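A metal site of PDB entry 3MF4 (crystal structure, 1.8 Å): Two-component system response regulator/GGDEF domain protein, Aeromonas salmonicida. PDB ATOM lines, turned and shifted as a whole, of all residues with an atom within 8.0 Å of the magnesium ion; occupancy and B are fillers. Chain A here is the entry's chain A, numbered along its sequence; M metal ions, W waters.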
ATOM      1  N   VAL A  10     -22.976 -27.114  22.309  1.00  0.00           N
ATOM      2  CA  VAL A  10     -22.536 -25.842  21.733  1.00  0.00           C
ATOM      3  C   VAL A  10     -21.165 -25.577  22.345  1.00  0.00           C
ATOM      4  O   VAL A  10     -21.059 -25.224  23.507  1.00  0.00           O
ATOM      5  CB  VAL A  10     -23.521 -24.692  21.999  1.00  0.00           C
ATOM      6  CG1 VAL A  10     -23.156 -23.453  21.141  1.00  0.00           C
ATOM      7  CG2 VAL A  10     -24.976 -25.107  21.717  1.00  0.00           C
ATOM      8  N   GLU A  11     -20.108 -25.809  21.576  1.00  0.00           N
ATOM      9  CA  GLU A  11     -18.749 -25.835  22.127  1.00  0.00           C
ATOM     10  C   GLU A  11     -17.807 -25.608  20.949  1.00  0.00           C
ATOM     11  O   GLU A  11     -17.817 -26.370  20.002  1.00  0.00           O
ATOM     12  CB  GLU A  11     -18.495 -27.194  22.821  1.00  0.00           C
ATOM     13  CG  GLU A  11     -17.025 -27.551  23.203  1.00  0.00           C
ATOM     14  CD  GLU A  11     -16.356 -26.567  24.135  1.00  0.00           C
ATOM     15  OE1 GLU A  11     -16.614 -26.630  25.347  1.00  0.00           O
ATOM     16  OE2 GLU A  11     -15.499 -25.781  23.657  1.00  0.00           O
ATOM     17  N   ASP A  12     -16.978 -24.567  21.014  1.00  0.00           N
ATOM     18  CA  ASP A  12     -16.090 -24.255  19.882  1.00  0.00           C
ATOM     19  C   ASP A  12     -14.773 -25.045  19.803  1.00  0.00           C
ATOM     20  O   ASP A  12     -14.132 -25.079  18.742  1.00  0.00           O
ATOM     21  CB  ASP A  12     -15.838 -22.754  19.760  1.00  0.00           C
ATOM     22  CG  ASP A  12     -15.187 -22.156  20.993  1.00  0.00           C
ATOM     23  OD1 ASP A  12     -14.384 -21.217  20.843  1.00  0.00           O
ATOM     24  OD2 ASP A  12     -15.507 -22.602  22.117  1.00  0.00           O
ATOM     25  N   SER A  13     -14.320 -25.612  20.926  1.00  0.00           N
ATOM     26  CA  SER A  13     -13.179 -26.513  20.873  1.00  0.00           C
ATOM     27  C   SER A  13     -13.458 -27.747  20.004  1.00  0.00           C
ATOM     28  O   SER A  13     -14.276 -28.596  20.370  1.00  0.00           O
ATOM     29  CB  SER A  13     -12.692 -26.927  22.261  1.00  0.00           C
ATOM     30  OG  SER A  13     -11.717 -27.929  22.127  1.00  0.00           O
ATOM     31  N   ILE A  16     -12.831 -30.898  22.148  1.00  0.00           N
ATOM     32  CA  ILE A  16     -13.842 -31.206  23.162  1.00  0.00           C
ATOM     33  C   ILE A  16     -15.153 -31.633  22.506  1.00  0.00           C
ATOM     34  O   ILE A  16     -15.792 -32.634  22.918  1.00  0.00           O
ATOM     35  CB  ILE A  16     -14.052 -30.043  24.155  1.00  0.00           C
ATOM     36  CG1 ILE A  16     -12.821 -29.931  25.051  1.00  0.00           C
ATOM     37  CG2 ILE A  16     -15.278 -30.303  25.064  1.00  0.00           C
ATOM     38  CD1 ILE A  16     -12.353 -28.510  25.347  1.00  0.00           C
ATOM     39  N   ASP A  36     -20.388 -25.068  16.736  1.00  0.00           N
ATOM     40  CA  ASP A  36     -19.225 -24.363  17.265  1.00  0.00           C
ATOM     41  C   ASP A  36     -19.533 -22.904  17.625  1.00  0.00           C
ATOM     42  O   ASP A  36     -18.647 -22.189  18.108  1.00  0.00           O
ATOM     43  CB  ASP A  36     -18.038 -24.461  16.292  1.00  0.00           C
ATOM     44  CG  ASP A  36     -18.336 -23.891  14.924  1.00  0.00           C
ATOM     45  OD1 ASP A  36     -19.384 -23.247  14.719  1.00  0.00           O
ATOM     46  OD2 ASP A  36     -17.491 -24.104  14.015  1.00  0.00           O
ATOM     47  N   VAL A  54     -23.298 -26.686  27.251  1.00  0.00           N
ATOM     48  CA  VAL A  54     -23.067 -25.302  26.801  1.00  0.00           C
ATOM     49  C   VAL A  54     -21.735 -24.750  27.310  1.00  0.00           C
ATOM     50  O   VAL A  54     -21.515 -24.682  28.519  1.00  0.00           O
ATOM     51  CB  VAL A  54     -24.226 -24.359  27.218  1.00  0.00           C
ATOM     52  CG1 VAL A  54     -23.952 -22.929  26.778  1.00  0.00           C
ATOM     53  CG2 VAL A  54     -25.587 -24.833  26.647  1.00  0.00           C
ATOM     54  N   ASP A  55     -20.876 -24.368  26.370  1.00  0.00           N
ATOM     55  CA  ASP A  55     -19.617 -23.715  26.660  1.00  0.00           C
ATOM     56  C   ASP A  55     -19.876 -22.254  27.022  1.00  0.00           C
ATOM     57  O   ASP A  55     -20.765 -21.591  26.449  1.00  0.00           O
ATOM     58  CB  ASP A  55     -18.724 -23.798  25.418  1.00  0.00           C
ATOM     59  CG  ASP A  55     -17.369 -23.196  25.610  1.00  0.00           C
ATOM     60  OD1 ASP A  55     -16.772 -23.280  26.705  1.00  0.00           O
ATOM     61  OD2 ASP A  55     -16.853 -22.680  24.621  1.00  0.00           O
ATOM     62  N   LEU A  56     -19.114 -21.768  27.997  1.00  0.00           N
ATOM     63  CA  LEU A  56     -19.143 -20.331  28.362  1.00  0.00           C
ATOM     64  C   LEU A  56     -18.206 -19.467  27.517  1.00  0.00           C
ATOM     65  O   LEU A  56     -18.314 -18.239  27.557  1.00  0.00           O
ATOM     66  CB  LEU A  56     -18.761 -20.150  29.833  1.00  0.00           C
ATOM     67  CG  LEU A  56     -19.495 -21.031  30.848  1.00  0.00           C
ATOM     68  CD1 LEU A  56     -18.896 -20.876  32.233  1.00  0.00           C
ATOM     69  CD2 LEU A  56     -20.961 -20.680  30.822  1.00  0.00           C
ATOM     70  N   THR A  57     -17.288 -20.085  26.777  1.00  0.00           N
ATOM     71  CA  THR A  57     -16.386 -19.340  25.878  1.00  0.00           C
ATOM     72  C   THR A  57     -16.703 -19.512  24.392  1.00  0.00           C
ATOM     73  O   THR A  57     -15.920 -20.116  23.649  1.00  0.00           O
ATOM     74  CB  THR A  57     -14.875 -19.681  26.131  1.00  0.00           C
ATOM     75  OG1 THR A  57     -14.629 -21.061  25.818  1.00  0.00           O
ATOM     76  CG2 THR A  57     -14.486 -19.399  27.557  1.00  0.00           C
ATOM     77  N   LEU A  58     -17.855 -19.028  23.928  1.00  0.00           N
ATOM     78  CA  LEU A  58     -18.159 -19.139  22.483  1.00  0.00           C
ATOM     79  C   LEU A  58     -17.747 -17.885  21.667  1.00  0.00           C
ATOM     80  O   LEU A  58     -17.704 -16.805  22.187  1.00  0.00           O
ATOM     81  CB  LEU A  58     -19.633 -19.457  22.282  1.00  0.00           C
ATOM     82  CG  LEU A  58     -20.008 -20.815  22.865  1.00  0.00           C
ATOM     83  CD1 LEU A  58     -21.515 -20.952  22.948  1.00  0.00           C
ATOM     84  CD2 LEU A  58     -19.356 -21.950  22.032  1.00  0.00           C
ATOM     85  N   PRO A  59     -17.451 -18.028  20.393  1.00  0.00           N
ATOM     86  CA  PRO A  59     -17.014 -16.882  19.640  1.00  0.00           C
ATOM     87  C   PRO A  59     -18.050 -15.760  19.558  1.00  0.00           C
ATOM     88  O   PRO A  59     -17.612 -14.658  19.417  1.00  0.00           O
ATOM     89  CB  PRO A  59     -16.781 -17.458  18.272  1.00  0.00           C
ATOM     90  CG  PRO A  59     -16.329 -18.724  18.481  1.00  0.00           C
ATOM     91  CD  PRO A  59     -17.231 -19.230  19.590  1.00  0.00           C
ATOM     92  N   ALA A  61     -20.535 -15.562  21.883  1.00  0.00           N
ATOM     93  CA  ALA A  61     -20.990 -15.527  23.233  1.00  0.00           C
ATOM     94  C   ALA A  61     -19.868 -15.946  24.157  1.00  0.00           C
ATOM     95  O   ALA A  61     -19.885 -17.011  24.728  1.00  0.00           O
ATOM     96  CB  ALA A  61     -22.151 -16.426  23.420  1.00  0.00           C
ATOM     97  N   PRO A  62     -18.905 -15.062  24.276  1.00  0.00           N
ATOM     98  CA  PRO A  62     -17.654 -15.347  24.996  1.00  0.00           C
ATOM     99  C   PRO A  62     -17.674 -15.260  26.484  1.00  0.00           C
ATOM    100  O   PRO A  62     -16.726 -15.544  27.108  1.00  0.00           O
ATOM    101  CB  PRO A  62     -16.731 -14.285  24.467  1.00  0.00           C
ATOM    102  CG  PRO A  62     -17.664 -13.176  24.135  1.00  0.00           C
ATOM    103  CD  PRO A  62     -18.817 -13.783  23.570  1.00  0.00           C
ATOM    104  N   LEU A  80     -20.444 -26.350  30.423  1.00  0.00           N
ATOM    105  CA  LEU A  80     -19.107 -26.907  30.275  1.00  0.00           C
ATOM    106  C   LEU A  80     -18.097 -25.854  30.729  1.00  0.00           C
ATOM    107  O   LEU A  80     -18.065 -24.765  30.196  1.00  0.00           O
ATOM    108  CB  LEU A  80     -18.832 -27.337  28.828  1.00  0.00           C
ATOM    109  CG  LEU A  80     -19.647 -28.488  28.234  1.00  0.00           C
ATOM    110  CD1 LEU A  80     -19.572 -28.472  26.703  1.00  0.00           C
ATOM    111  CD2 LEU A  80     -19.167 -29.835  28.772  1.00  0.00           C
ATOM    112  N   LYS A 103     -14.337 -29.538  32.187  1.00  0.00           N
ATOM    113  CA  LYS A 103     -13.785 -29.986  30.899  1.00  0.00           C
ATOM    114  C   LYS A 103     -12.287 -29.747  30.837  1.00  0.00           C
ATOM    115  O   LYS A 103     -11.714 -29.574  29.747  1.00  0.00           O
ATOM    116  CB  LYS A 103     -14.526 -29.327  29.720  1.00  0.00           C
ATOM    117  CG  LYS A 103     -14.450 -27.816  29.706  1.00  0.00           C
ATOM    118  CD  LYS A 103     -14.496 -27.258  28.301  1.00  0.00           C
ATOM    119  CE  LYS A 103     -14.794 -25.777  28.374  1.00  0.00           C
ATOM    120  NZ  LYS A 103     -14.821 -25.202  27.003  1.00  0.00           N
HETATM  121 MG    MG M   1     -15.008 -22.038  23.988  1.00  0.00          MG
HETATM  122  O   HOH W   1     -14.126 -23.719  24.446  1.00  0.00           O
HETATM  123  O   HOH W   2     -13.248 -21.081  23.109  1.00  0.00           O
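Merely in contact with the magnesium ion: Glu 11.
The side-chain carboxylate (OE2) of Glu 11 lies within hydrogen-bond range of the backbone NH (N) of Ser 13 (3.0 Å). O of Val 10 is in hydrogen-bond range of N of Asp 55, 3.0 Å away. The side-chain carboxylate (OE1) of Glu 11 lies within salt-bridge range of the side-chain amino group (NZ) of Lys 103, 2.8 Å away. OD1 of Asp 55 lies within salt-bridge range of NZ of Lys 103 (2.8 Å).
Water W1 bridges OE2 of Glu 11 and NZ of Lys 103.
The magnesium ion is bound by water W1 (2.0 Å), OD2 of Asp 12 (2.0 Å), OD2 of Asp 55 (2.1 Å), OG1 of Thr 57 (2.1 Å), O of Thr 57 (2.2 Å) and water W2 (2.2 Å).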
